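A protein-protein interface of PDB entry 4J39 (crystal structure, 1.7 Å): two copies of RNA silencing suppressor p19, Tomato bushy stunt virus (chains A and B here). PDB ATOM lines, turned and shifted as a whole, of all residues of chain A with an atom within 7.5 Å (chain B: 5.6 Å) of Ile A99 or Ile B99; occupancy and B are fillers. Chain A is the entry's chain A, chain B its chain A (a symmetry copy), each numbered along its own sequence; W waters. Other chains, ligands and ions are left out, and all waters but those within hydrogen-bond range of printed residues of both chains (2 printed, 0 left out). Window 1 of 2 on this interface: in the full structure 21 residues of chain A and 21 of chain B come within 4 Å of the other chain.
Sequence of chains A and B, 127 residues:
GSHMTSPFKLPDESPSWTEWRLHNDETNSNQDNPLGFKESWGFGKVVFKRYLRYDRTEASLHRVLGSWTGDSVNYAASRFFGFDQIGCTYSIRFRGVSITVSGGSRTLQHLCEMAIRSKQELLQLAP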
ATOM      1  N   LYS A  38     -16.100  20.869   8.843  1.00  0.00           N
ATOM      2  CA  LYS A  38     -15.612  21.333  10.113  1.00  0.00           C
ATOM      3  C   LYS A  38     -16.731  21.549  11.101  1.00  0.00           C
ATOM      4  O   LYS A  38     -17.814  22.096  10.775  1.00  0.00           O
ATOM      5  CB  LYS A  38     -14.854  22.663   9.859  1.00  0.00           C
ATOM      6  CG  LYS A  38     -13.547  22.760   9.066  1.00  0.00           C
ATOM      7  CD  LYS A  38     -13.002  24.219   8.891  1.00  0.00           C
ATOM      8  CE  LYS A  38     -13.468  24.901   7.633  1.00  0.00           C
ATOM      9  NZ  LYS A  38     -12.831  24.270   6.437  1.00  0.00           N
ATOM     10  N   SER A  40     -17.430  22.707  15.480  1.00  0.00           N
ATOM     11  CA  SER A  40     -16.886  23.242  16.744  1.00  0.00           C
ATOM     12  C   SER A  40     -17.896  23.399  17.845  1.00  0.00           C
ATOM     13  O   SER A  40     -19.090  23.581  17.627  1.00  0.00           O
ATOM     14  CB  SER A  40     -16.185  24.571  16.407  1.00  0.00           C
ATOM     15  OG  SER A  40     -17.140  25.506  16.115  1.00  0.00           O
ATOM     16  N   THR A  89     -22.149  27.342  22.127  1.00  0.00           N
ATOM     17  CA  THR A  89     -22.331  27.402  20.683  1.00  0.00           C
ATOM     18  C   THR A  89     -21.806  26.207  19.949  1.00  0.00           C
ATOM     19  O   THR A  89     -20.650  25.752  20.153  1.00  0.00           O
ATOM     20  CB  THR A  89     -21.657  28.669  20.042  1.00  0.00           C
ATOM     21  OG1 THR A  89     -22.158  29.848  20.613  1.00  0.00           O
ATOM     22  CG2 THR A  89     -21.994  28.819  18.622  1.00  0.00           C
ATOM     23  N   TYR A  90     -22.646  25.645  19.038  1.00  0.00           N
ATOM     24  CA  TYR A  90     -22.163  24.606  18.151  1.00  0.00           C
ATOM     25  C   TYR A  90     -22.167  25.186  16.723  1.00  0.00           C
ATOM     26  O   TYR A  90     -23.133  25.914  16.377  1.00  0.00           O
ATOM     27  CB  TYR A  90     -23.121  23.360  18.193  1.00  0.00           C
ATOM     28  CG  TYR A  90     -22.726  22.360  17.166  1.00  0.00           C
ATOM     29  CD1 TYR A  90     -21.559  21.581  17.233  1.00  0.00           C
ATOM     30  CD2 TYR A  90     -23.489  22.213  15.992  1.00  0.00           C
ATOM     31  CE1 TYR A  90     -21.213  20.640  16.336  1.00  0.00           C
ATOM     32  CE2 TYR A  90     -23.140  21.327  14.992  1.00  0.00           C
ATOM     33  CZ  TYR A  90     -22.005  20.528  15.100  1.00  0.00           C
ATOM     34  OH  TYR A  90     -21.625  19.610  14.200  1.00  0.00           O
ATOM     35  N   SER A  91     -21.137  24.977  15.962  1.00  0.00           N
ATOM     36  CA  SER A  91     -21.095  25.349  14.547  1.00  0.00           C
ATOM     37  C   SER A  91     -20.664  24.237  13.686  1.00  0.00           C
ATOM     38  O   SER A  91     -19.809  23.443  14.050  1.00  0.00           O
ATOM     39  CB  SER A  91     -20.109  26.438  14.405  1.00  0.00           C
ATOM     40  OG  SER A  91     -20.500  27.338  13.360  1.00  0.00           O
ATOM     41  N   ILE A  92     -21.204  24.152  12.469  1.00  0.00           N
ATOM     42  CA  ILE A  92     -20.775  23.216  11.509  1.00  0.00           C
ATOM     43  C   ILE A  92     -20.767  23.921  10.088  1.00  0.00           C
ATOM     44  O   ILE A  92     -21.668  24.766   9.833  1.00  0.00           O
ATOM     45  CB  ILE A  92     -21.672  21.951  11.420  1.00  0.00           C
ATOM     46  CG1 ILE A  92     -21.072  20.970  10.436  1.00  0.00           C
ATOM     47  CG2 ILE A  92     -23.177  22.313  11.350  1.00  0.00           C
ATOM     48  CD1 ILE A  92     -21.845  19.562  10.534  1.00  0.00           C
ATOM     49  N   ARG A  93     -19.753  23.661   9.289  1.00  0.00           N
ATOM     50  CA  ARG A  93     -19.661  24.162   7.966  1.00  0.00           C
ATOM     51  C   ARG A  93     -19.367  23.027   6.964  1.00  0.00           C
ATOM     52  O   ARG A  93     -18.443  22.185   7.170  1.00  0.00           O
ATOM     53  CB  ARG A  93     -18.590  25.240   7.891  1.00  0.00           C
ATOM     54  CG  ARG A  93     -18.354  25.660   6.467  1.00  0.00           C
ATOM     55  CD  ARG A  93     -17.952  27.023   6.340  1.00  0.00           C
ATOM     56  NE  ARG A  93     -17.779  27.427   4.933  1.00  0.00           N
ATOM     57  CZ  ARG A  93     -17.485  28.663   4.560  1.00  0.00           C
ATOM     58  NH1 ARG A  93     -17.349  29.605   5.486  1.00  0.00           N
ATOM     59  NH2 ARG A  93     -17.284  28.959   3.288  1.00  0.00           N
ATOM     60  N   PHE A  94     -20.208  22.974   5.918  1.00  0.00           N
ATOM     61  CA  PHE A  94     -20.043  21.977   4.870  1.00  0.00           C
ATOM     62  C   PHE A  94     -20.535  22.564   3.531  1.00  0.00           C
ATOM     63  O   PHE A  94     -21.638  23.146   3.488  1.00  0.00           O
ATOM     64  CB  PHE A  94     -20.822  20.726   5.264  1.00  0.00           C
ATOM     65  CG  PHE A  94     -20.647  19.594   4.326  1.00  0.00           C
ATOM     66  CD1 PHE A  94     -19.396  19.107   3.965  1.00  0.00           C
ATOM     67  CD2 PHE A  94     -21.817  18.966   3.780  1.00  0.00           C
ATOM     68  CE1 PHE A  94     -19.269  17.977   3.093  1.00  0.00           C
ATOM     69  CE2 PHE A  94     -21.685  17.920   2.890  1.00  0.00           C
ATOM     70  CZ  PHE A  94     -20.454  17.422   2.566  1.00  0.00           C
ATOM     71  N   VAL A  97     -22.068  26.218   3.350  1.00  0.00           N
ATOM     72  CA  VAL A  97     -23.086  26.615   4.282  1.00  0.00           C
ATOM     73  C   VAL A  97     -22.674  26.309   5.734  1.00  0.00           C
ATOM     74  O   VAL A  97     -22.163  25.214   6.011  1.00  0.00           O
ATOM     75  CB  VAL A  97     -24.572  26.089   3.967  1.00  0.00           C
ATOM     76  CG1 VAL A  97     -24.865  25.460   2.496  1.00  0.00           C
ATOM     77  CG2 VAL A  97     -25.491  25.893   5.148  1.00  0.00           C
ATOM     78  N   SER A  98     -22.825  27.331   6.565  1.00  0.00           N
ATOM     79  CA  SER A  98     -22.542  27.277   8.013  1.00  0.00           C
ATOM     80  C   SER A  98     -23.856  27.344   8.761  1.00  0.00           C
ATOM     81  O   SER A  98     -24.770  28.111   8.404  1.00  0.00           O
ATOM     82  CB  SER A  98     -21.692  28.476   8.317  1.00  0.00           C
ATOM     83  OG  SER A  98     -21.587  28.608   9.662  1.00  0.00           O
ATOM     84  N   ILE A  99     -24.010  26.446   9.736  1.00  0.00           N
ATOM     85  CA  ILE A  99     -25.070  26.481  10.687  1.00  0.00           C
ATOM     86  C   ILE A  99     -24.505  26.667  12.104  1.00  0.00           C
ATOM     87  O   ILE A  99     -23.603  25.908  12.538  1.00  0.00           O
ATOM     88  CB  ILE A  99     -25.976  25.248  10.623  1.00  0.00           C
ATOM     89  CG1 ILE A  99     -26.469  25.085   9.143  1.00  0.00           C
ATOM     90  CG2 ILE A  99     -27.120  25.321  11.614  1.00  0.00           C
ATOM     91  CD1 ILE A  99     -27.400  23.791   8.957  1.00  0.00           C
ATOM     92  N   THR A 100     -25.052  27.585  12.850  1.00  0.00           N
ATOM     93  CA  THR A 100     -24.614  27.773  14.241  1.00  0.00           C
ATOM     94  C   THR A 100     -25.841  27.646  15.185  1.00  0.00           C
ATOM     95  O   THR A 100     -26.891  28.242  14.990  1.00  0.00           O
ATOM     96  CB  THR A 100     -23.897  29.087  14.434  1.00  0.00           C
ATOM     97  OG1 THR A 100     -22.749  29.126  13.579  1.00  0.00           O
ATOM     98  CG2 THR A 100     -23.472  29.312  15.865  1.00  0.00           C
ATOM     99  N   VAL A 101     -25.715  26.950  16.299  1.00  0.00           N
ATOM    100  CA  VAL A 101     -26.753  26.806  17.214  1.00  0.00           C
ATOM    101  C   VAL A 101     -26.221  27.314  18.553  1.00  0.00           C
ATOM    102  O   VAL A 101     -25.190  26.827  19.022  1.00  0.00           O
ATOM    103  CB  VAL A 101     -27.216  25.261  17.416  1.00  0.00           C
ATOM    104  CG1 VAL A 101     -28.319  25.058  18.519  1.00  0.00           C
ATOM    105  CG2 VAL A 101     -27.580  24.533  16.111  1.00  0.00           C
ATOM    106  N   SER A 102     -26.892  28.297  19.144  1.00  0.00           N
ATOM    107  CA  SER A 102     -26.284  29.037  20.307  1.00  0.00           C
ATOM    108  C   SER A 102     -27.319  29.318  21.388  1.00  0.00           C
ATOM    109  O   SER A 102     -28.546  29.550  21.104  1.00  0.00           O
ATOM    110  CB  SER A 102     -25.629  30.366  19.826  1.00  0.00           C
ATOM    111  OG  SER A 102     -26.432  31.099  18.966  1.00  0.00           O
ATOM    112  N   HIS A 110     -31.257  21.248  24.972  1.00  0.00           N
ATOM    113  CA  HIS A 110     -31.978  21.660  23.747  1.00  0.00           C
ATOM    114  C   HIS A 110     -30.971  22.134  22.681  1.00  0.00           C
ATOM    115  O   HIS A 110     -31.185  21.873  21.484  1.00  0.00           O
ATOM    116  CB  HIS A 110     -32.971  22.787  24.049  1.00  0.00           C
ATOM    117  CG  HIS A 110     -34.171  22.399  24.854  1.00  0.00           C
ATOM    118  ND1 HIS A 110     -34.750  21.139  24.822  1.00  0.00           N
ATOM    119  CD2 HIS A 110     -34.976  23.161  25.630  1.00  0.00           C
ATOM    120  CE1 HIS A 110     -35.821  21.129  25.607  1.00  0.00           C
ATOM    121  NE2 HIS A 110     -35.985  22.351  26.098  1.00  0.00           N
ATOM    122  N   LEU A 111     -29.871  22.830  23.054  1.00  0.00           N
ATOM    123  CA  LEU A 111     -28.876  23.130  22.052  1.00  0.00           C
ATOM    124  C   LEU A 111     -28.307  21.825  21.412  1.00  0.00           C
ATOM    125  O   LEU A 111     -28.149  21.770  20.201  1.00  0.00           O
ATOM    126  CB  LEU A 111     -27.734  24.003  22.570  1.00  0.00           C
ATOM    127  CG  LEU A 111     -28.107  25.276  23.235  1.00  0.00           C
ATOM    128  CD1 LEU A 111     -26.815  25.873  23.950  1.00  0.00           C
ATOM    129  CD2 LEU A 111     -28.719  26.239  22.241  1.00  0.00           C
ATOM    130  N   MET A 114     -30.907  20.337  18.941  1.00  0.00           N
ATOM    131  CA  MET A 114     -30.955  21.074  17.663  1.00  0.00           C
ATOM    132  C   MET A 114     -29.646  20.938  16.881  1.00  0.00           C
ATOM    133  O   MET A 114     -29.657  20.902  15.621  1.00  0.00           O
ATOM    134  CB  MET A 114     -31.289  22.575  17.860  1.00  0.00           C
ATOM    135  CG  MET A 114     -32.653  22.873  18.470  1.00  0.00           C
ATOM    136  SD  MET A 114     -33.988  22.055  17.458  1.00  0.00           S
ATOM    137  CE  MET A 114     -33.562  22.349  15.817  1.00  0.00           C
ATOM    138  N   ALA A 115     -28.516  20.894  17.567  1.00  0.00           N
ATOM    139  CA  ALA A 115     -27.190  20.753  16.934  1.00  0.00           C
ATOM    140  C   ALA A 115     -27.097  19.406  16.155  1.00  0.00           C
ATOM    141  O   ALA A 115     -26.640  19.365  15.038  1.00  0.00           O
ATOM    142  CB  ALA A 115     -26.078  20.851  18.029  1.00  0.00           C
ATOM    143  N   ARG A 117     -29.510  17.507  14.963  1.00  0.00           N
ATOM    144  CA  ARG A 117     -30.532  17.541  13.878  1.00  0.00           C
ATOM    145  C   ARG A 117     -29.929  18.412  12.732  1.00  0.00           C
ATOM    146  O   ARG A 117     -29.911  18.023  11.542  1.00  0.00           O
ATOM    147  CB  ARG A 117     -31.867  18.125  14.380  1.00  0.00           C
ATOM    148  CG  ARG A 117     -32.660  17.298  15.380  1.00  0.00           C
ATOM    149  CD  ARG A 117     -34.084  17.893  15.706  1.00  0.00           C
ATOM    150  NE  ARG A 117     -34.913  17.162  16.690  1.00  0.00           N
ATOM    151  CZ  ARG A 117     -34.436  16.363  17.694  1.00  0.00           C
ATOM    152  NH1 ARG A 117     -33.109  16.120  17.936  1.00  0.00           N
ATOM    153  NH2 ARG A 117     -35.303  15.819  18.526  1.00  0.00           N
ATOM    154  N   SER A 118     -29.283  19.525  13.121  1.00  0.00           N
ATOM    155  CA  SER A 118     -28.657  20.414  12.093  1.00  0.00           C
ATOM    156  C   SER A 118     -27.553  19.745  11.321  1.00  0.00           C
ATOM    157  O   SER A 118     -27.420  19.843  10.096  1.00  0.00           O
ATOM    158  CB  SER A 118     -28.046  21.633  12.813  1.00  0.00           C
ATOM    159  OG  SER A 118     -29.027  22.509  13.365  1.00  0.00           O
ATOM    160  N   LYS A 119     -26.710  19.077  12.090  1.00  0.00           N
ATOM    161  CA  LYS A 119     -25.590  18.356  11.537  1.00  0.00           C
ATOM    162  C   LYS A 119     -26.136  17.293  10.518  1.00  0.00           C
ATOM    163  O   LYS A 119     -25.627  17.184   9.462  1.00  0.00           O
ATOM    164  CB  LYS A 119     -24.771  17.611  12.641  1.00  0.00           C
ATOM    165  CG  LYS A 119     -23.606  16.866  12.148  1.00  0.00           C
ATOM    166  CD  LYS A 119     -22.834  16.268  13.386  1.00  0.00           C
ATOM    167  CE  LYS A 119     -21.553  15.591  13.082  1.00  0.00           C
ATOM    168  NZ  LYS A 119     -20.781  15.290  14.387  1.00  0.00           N
ATOM    169  N   GLU A 121     -28.913  17.126   8.854  1.00  0.00           N
ATOM    170  CA  GLU A 121     -29.591  17.680   7.653  1.00  0.00           C
ATOM    171  C   GLU A 121     -28.594  18.305   6.727  1.00  0.00           C
ATOM    172  O   GLU A 121     -28.673  18.153   5.500  1.00  0.00           O
ATOM    173  CB  GLU A 121     -30.685  18.659   8.099  1.00  0.00           C
ATOM    174  CG  GLU A 121     -31.726  17.946   9.103  1.00  0.00           C
ATOM    175  CD  GLU A 121     -33.208  17.656   8.644  1.00  0.00           C
ATOM    176  OE1 GLU A 121     -33.941  18.593   8.192  1.00  0.00           O
ATOM    177  OE2 GLU A 121     -33.610  16.475   8.830  1.00  0.00           O
ATOM    178  N   LEU A 122     -27.568  18.980   7.291  1.00  0.00           N
ATOM    179  CA  LEU A 122     -26.542  19.551   6.429  1.00  0.00           C
ATOM    180  C   LEU A 122     -25.717  18.543   5.658  1.00  0.00           C
ATOM    181  O   LEU A 122     -25.424  18.674   4.453  1.00  0.00           O
ATOM    182  CB  LEU A 122     -25.590  20.466   7.298  1.00  0.00           C
ATOM    183  CG  LEU A 122     -24.578  21.221   6.511  1.00  0.00           C
ATOM    184  CD1 LEU A 122     -25.138  22.089   5.291  1.00  0.00           C
ATOM    185  CD2 LEU A 122     -23.681  22.160   7.455  1.00  0.00           C
ATOM    186  N   LEU A 123     -25.322  17.484   6.362  1.00  0.00           N
ATOM    187  CA  LEU A 123     -24.488  16.445   5.799  1.00  0.00           C
ATOM    188  C   LEU A 123     -25.298  15.596   4.756  1.00  0.00           C
ATOM    189  O   LEU A 123     -24.711  15.077   3.827  1.00  0.00           O
ATOM    190  CB  LEU A 123     -23.879  15.593   6.914  1.00  0.00           C
ATOM    191  CG  LEU A 123     -22.901  16.324   7.858  1.00  0.00           C
ATOM    192  CD1 LEU A 123     -22.365  15.261   8.988  1.00  0.00           C
ATOM    193  CD2 LEU A 123     -21.797  16.983   7.031  1.00  0.00           C
ATOM    194  N   TYR B  90     -29.653  33.712   7.638  1.00  0.00           N
ATOM    195  CA  TYR B  90     -30.974  33.593   8.219  1.00  0.00           C
ATOM    196  C   TYR B  90     -30.787  33.266   9.714  1.00  0.00           C
ATOM    197  O   TYR B  90     -29.877  32.460  10.041  1.00  0.00           O
ATOM    198  CB  TYR B  90     -31.768  32.417   7.541  1.00  0.00           C
ATOM    199  CG  TYR B  90     -33.058  32.182   8.244  1.00  0.00           C
ATOM    200  CD1 TYR B  90     -34.149  33.065   8.204  1.00  0.00           C
ATOM    201  CD2 TYR B  90     -33.211  31.063   9.085  1.00  0.00           C
ATOM    202  CE1 TYR B  90     -35.337  32.842   8.796  1.00  0.00           C
ATOM    203  CE2 TYR B  90     -34.374  30.824   9.789  1.00  0.00           C
ATOM    204  CZ  TYR B  90     -35.462  31.687   9.698  1.00  0.00           C
ATOM    205  OH  TYR B  90     -36.642  31.500  10.307  1.00  0.00           O
ATOM    206  N   SER B  91     -31.512  33.896  10.587  1.00  0.00           N
ATOM    207  CA  SER B  91     -31.525  33.563  12.011  1.00  0.00           C
ATOM    208  C   SER B  91     -32.889  33.388  12.534  1.00  0.00           C
ATOM    209  O   SER B  91     -33.817  34.081  12.143  1.00  0.00           O
ATOM    210  CB  SER B  91     -30.907  34.692  12.736  1.00  0.00           C
ATOM    211  OG  SER B  91     -30.205  34.222  13.894  1.00  0.00           O
ATOM    212  N   ILE B  92     -33.072  32.472  13.488  1.00  0.00           N
ATOM    213  CA  ILE B  92     -34.299  32.307  14.159  1.00  0.00           C
ATOM    214  C   ILE B  92     -34.000  32.025  15.691  1.00  0.00           C
ATOM    215  O   ILE B  92     -32.985  31.338  15.987  1.00  0.00           O
ATOM    216  CB  ILE B  92     -35.163  31.139  13.607  1.00  0.00           C
ATOM    217  CG1 ILE B  92     -36.494  31.107  14.327  1.00  0.00           C
ATOM    218  CG2 ILE B  92     -34.335  29.841  13.432  1.00  0.00           C
ATOM    219  CD1 ILE B  92     -37.486  30.078  13.587  1.00  0.00           C
ATOM    220  N   ARG B  93     -34.775  32.616  16.577  1.00  0.00           N
ATOM    221  CA  ARG B  93     -34.667  32.392  17.972  1.00  0.00           C
ATOM    222  C   ARG B  93     -36.038  32.038  18.583  1.00  0.00           C
ATOM    223  O   ARG B  93     -37.071  32.730  18.338  1.00  0.00           O
ATOM    224  CB  ARG B  93     -34.072  33.615  18.652  1.00  0.00           C
ATOM    225  CG  ARG B  93     -34.112  33.467  20.148  1.00  0.00           C
ATOM    226  CD  ARG B  93     -33.041  34.139  20.809  1.00  0.00           C
ATOM    227  NE  ARG B  93     -33.069  33.935  22.270  1.00  0.00           N
ATOM    228  CZ  ARG B  93     -32.136  34.396  23.088  1.00  0.00           C
ATOM    229  NH1 ARG B  93     -31.105  35.065  22.586  1.00  0.00           N
ATOM    230  NH2 ARG B  93     -32.239  34.233  24.395  1.00  0.00           N
ATOM    231  N   VAL B  97     -33.077  29.206  22.291  1.00  0.00           N
ATOM    232  CA  VAL B  97     -32.145  28.690  21.329  1.00  0.00           C
ATOM    233  C   VAL B  97     -32.217  29.466  20.000  1.00  0.00           C
ATOM    234  O   VAL B  97     -33.321  29.741  19.506  1.00  0.00           O
ATOM    235  CB  VAL B  97     -32.189  27.102  21.088  1.00  0.00           C
ATOM    236  CG1 VAL B  97     -33.012  26.189  22.153  1.00  0.00           C
ATOM    237  CG2 VAL B  97     -31.771  26.606  19.725  1.00  0.00           C
ATOM    238  N   SER B  98     -31.038  29.864  19.542  1.00  0.00           N
ATOM    239  CA  SER B  98     -30.839  30.585  18.269  1.00  0.00           C
ATOM    240  C   SER B  98     -30.150  29.654  17.295  1.00  0.00           C
ATOM    241  O   SER B  98     -29.225  28.903  17.656  1.00  0.00           O
ATOM    242  CB  SER B  98     -29.968  31.764  18.590  1.00  0.00           C
ATOM    243  OG  SER B  98     -29.563  32.337  17.431  1.00  0.00           O
ATOM    244  N   ILE B  99     -30.680  29.607  16.071  1.00  0.00           N
ATOM    245  CA  ILE B  99     -30.058  28.967  14.961  1.00  0.00           C
ATOM    246  C   ILE B  99     -29.744  29.995  13.863  1.00  0.00           C
ATOM    247  O   ILE B  99     -30.638  30.765  13.432  1.00  0.00           O
ATOM    248  CB  ILE B  99     -30.883  27.807  14.396  1.00  0.00           C
ATOM    249  CG1 ILE B  99     -31.216  26.829  15.576  1.00  0.00           C
ATOM    250  CG2 ILE B  99     -30.189  27.113  13.242  1.00  0.00           C
ATOM    251  CD1 ILE B  99     -32.117  25.592  15.097  1.00  0.00           C
ATOM    252  N   THR B 100     -28.545  29.979  13.354  1.00  0.00           N
ATOM    253  CA  THR B 100     -28.192  30.884  12.250  1.00  0.00           C
ATOM    254  C   THR B 100     -27.661  30.049  11.053  1.00  0.00           C
ATOM    255  O   THR B 100     -26.807  29.182  11.176  1.00  0.00           O
ATOM    256  CB  THR B 100     -27.196  31.936  12.679  1.00  0.00           C
ATOM    257  OG1 THR B 100     -27.758  32.707  13.747  1.00  0.00           O
ATOM    258  CG2 THR B 100     -26.796  32.851  11.548  1.00  0.00           C
ATOM    259  N   VAL B 101     -28.070  30.353   9.836  1.00  0.00           N
ATOM    260  CA  VAL B 101     -27.628  29.674   8.705  1.00  0.00           C
ATOM    261  C   VAL B 101     -27.028  30.731   7.777  1.00  0.00           C
ATOM    262  O   VAL B 101     -27.711  31.697   7.435  1.00  0.00           O
ATOM    263  CB  VAL B 101     -28.824  28.926   7.901  1.00  0.00           C
ATOM    264  CG1 VAL B 101     -28.368  28.236   6.563  1.00  0.00           C
ATOM    265  CG2 VAL B 101     -29.673  27.978   8.765  1.00  0.00           C
ATOM    266  N   SER B 102     -25.764  30.566   7.402  1.00  0.00           N
ATOM    267  CA  SER B 102     -25.022  31.693   6.728  1.00  0.00           C
ATOM    268  C   SER B 102     -24.154  31.180   5.587  1.00  0.00           C
ATOM    269  O   SER B 102     -23.590  30.031   5.630  1.00  0.00           O
ATOM    270  CB  SER B 102     -24.154  32.468   7.763  1.00  0.00           C
ATOM    271  OG  SER B 102     -23.417  31.643   8.599  1.00  0.00           O
ATOM    272  N   MET B 114     -31.671  24.816   4.001  1.00  0.00           N
ATOM    273  CA  MET B 114     -31.290  24.539   5.400  1.00  0.00           C
ATOM    274  C   MET B 114     -32.049  25.436   6.382  1.00  0.00           C
ATOM    275  O   MET B 114     -32.378  25.001   7.518  1.00  0.00           O
ATOM    276  CB  MET B 114     -29.764  24.684   5.635  1.00  0.00           C
ATOM    277  CG  MET B 114     -28.881  23.723   4.851  1.00  0.00           C
ATOM    278  SD  MET B 114     -29.409  21.966   5.186  1.00  0.00           S
ATOM    279  CE  MET B 114     -29.680  21.887   6.884  1.00  0.00           C
ATOM    280  N   SER B 118     -34.355  24.163   9.437  1.00  0.00           N
ATOM    281  CA  SER B 118     -34.007  24.619  10.818  1.00  0.00           C
ATOM    282  C   SER B 118     -35.177  25.197  11.566  1.00  0.00           C
ATOM    283  O   SER B 118     -35.426  24.940  12.748  1.00  0.00           O
ATOM    284  CB  SER B 118     -32.936  25.725  10.709  1.00  0.00           C
ATOM    285  OG  SER B 118     -31.673  25.239  10.259  1.00  0.00           O
ATOM    286  N   LEU B 122     -36.830  23.658  14.990  1.00  0.00           N
ATOM    287  CA  LEU B 122     -36.867  24.452  16.211  1.00  0.00           C
ATOM    288  C   LEU B 122     -38.251  24.689  16.780  1.00  0.00           C
ATOM    289  O   LEU B 122     -38.520  24.592  17.993  1.00  0.00           O
ATOM    290  CB  LEU B 122     -36.155  25.838  15.946  1.00  0.00           C
ATOM    291  CG  LEU B 122     -36.004  26.691  17.157  1.00  0.00           C
ATOM    292  CD1 LEU B 122     -35.314  26.001  18.423  1.00  0.00           C
ATOM    293  CD2 LEU B 122     -35.232  28.058  16.819  1.00  0.00           C
HETATM  294  O   HOH W   1     -26.875  30.844  16.450  1.00  0.00           O
HETATM  295  O   HOH W   2     -24.099  30.344  10.706  1.00  0.00           O
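Of chain A, only Ile A99 (3.9 Å), Thr A100 (3.2 Å) and Met A114 (3.6 Å) come within 4 Å of Ile B99. Of the printed residues of chain B, Glu A121 touches Met B114 (3.6 Å). Of the printed residues of chain B, His A110 touches Val B97 (3.9 Å). Of the printed residues of chain B, Met A114 touches Ile B99 (3.6 Å) and Leu B122 (3.6 Å). Ser A40 touches none of the printed residues of chain B. The nearest residue of chain A that does not touch Ile B99 is Val A101 (4.3 Å).
Ser A98 touches Thr B100 (O to O, 3.6 Å). CA of Val B101 touches O of Ser A98, 3.3 Å away. CG2 of Ile A99 touches CG2 of Ile B99, 3.9 Å away. Thr B100 touches Ile A99. Met B114 touches Ile A99 (CE to CD1, 3.6 Å). O of Ser B98 touches O of Thr A100, at 3.6 Å. Thr A100 touches Ile B99 (O to CA, 3.2 Å). Val A101 touches Val B97. His A110 touches Val B97. CE of Met B114 touches N of Leu A122 (3.6 Å).
The backbone NH of Val A101 sits at hydrogen-bond distance from the backbone carbonyl oxygen of Tyr A90, 2.8 Å away. The side-chain hydroxyl (OG) of Ser A91 sits at hydrogen-bond distance from the side-chain hydroxyl (OG1) of Thr A100, 2.9 Å away. The backbone carbonyl oxygen (O) of Met A114 sits at hydrogen-bond distance from the side-chain hydroxyl (OG) of Ser A118. O of Tyr B90 is in hydrogen-bond range of N of Val B101 (2.8 Å). The side-chain hydroxyl of Thr B100 is in hydrogen-bond range of the side-chain hydroxyl of Ser B91, 2.9 Å away. The side-chain hydroxyl of Ser B118 is in hydrogen-bond range of the backbone carbonyl oxygen of Met B114.
Val A97 touches Ser B102, and with the chains exchanged Ser A102 touches Val B97. Ser A98 touches Thr B100, and with the chains exchanged Thr A100 touches Ser B98. Ile B99 touches its own counterpart, Ile A99. Met A114 touches Leu B122, and with the chains exchanged Leu A122 touches Met B114. 13 positions are printed for both chains. Of the 21 pairs that touch across the chains among the printed residues, 18 have their exchanged pair printed and touching as well.
Of the 13 printed residues of chain B, 8 touch a printed residue of chain A. Printed residues of chain B that touch a printed residue of chain A: Val B97, Ser B98, Ile B99, Thr B100, Val B101, Ser B102, Met B114 and Leu B122. Hydrophobic or aromatic side chains of chain B within 4 Å of the printed part of chain A: Val B97, Ile B99, Val B101 and Met B114. Hydrophobic or aromatic side chains of chain A within 4 Å of the printed part of chain B: Val A97, Ile A99, Val A101, His A110, Leu A111 and Met A114. Among the printed residues, 21 pairs touch across the chains. Among the printed residues, no Asp or Glu carboxylate lies within 4 Å of a Lys or Arg side-chain nitrogen of the other chain.
The backbone NH (N) of Ser B102 lies within hydrogen-bond range of the backbone carbonyl oxygen (O) of Ser A98, 2.8 Å away. The backbone NH of Thr B100 sits at hydrogen-bond distance from the backbone carbonyl oxygen of Thr A100 (2.9 Å). The backbone NH (N) of Ser A102 lies within hydrogen-bond range of the backbone carbonyl oxygen (O) of Ser B98.
Water W1 lies within hydrogen-bond range of the side-chain hydroxyl of Ser A102 (2.6 Å), the backbone carbonyl oxygen of Thr A100 (3.0 Å), the side-chain hydroxyl of Ser B98 (3.2 Å) and the side-chain hydroxyl of Thr B100 (3.4 Å). Water W2 lies within hydrogen-bond range of the side-chain hydroxyl of Ser B102 (2.6 Å), the backbone carbonyl oxygen of Thr B100 (3.0 Å), the side-chain hydroxyl of Ser A98 (3.2 Å) and the side-chain hydroxyl of Thr A100 (3.4 Å).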
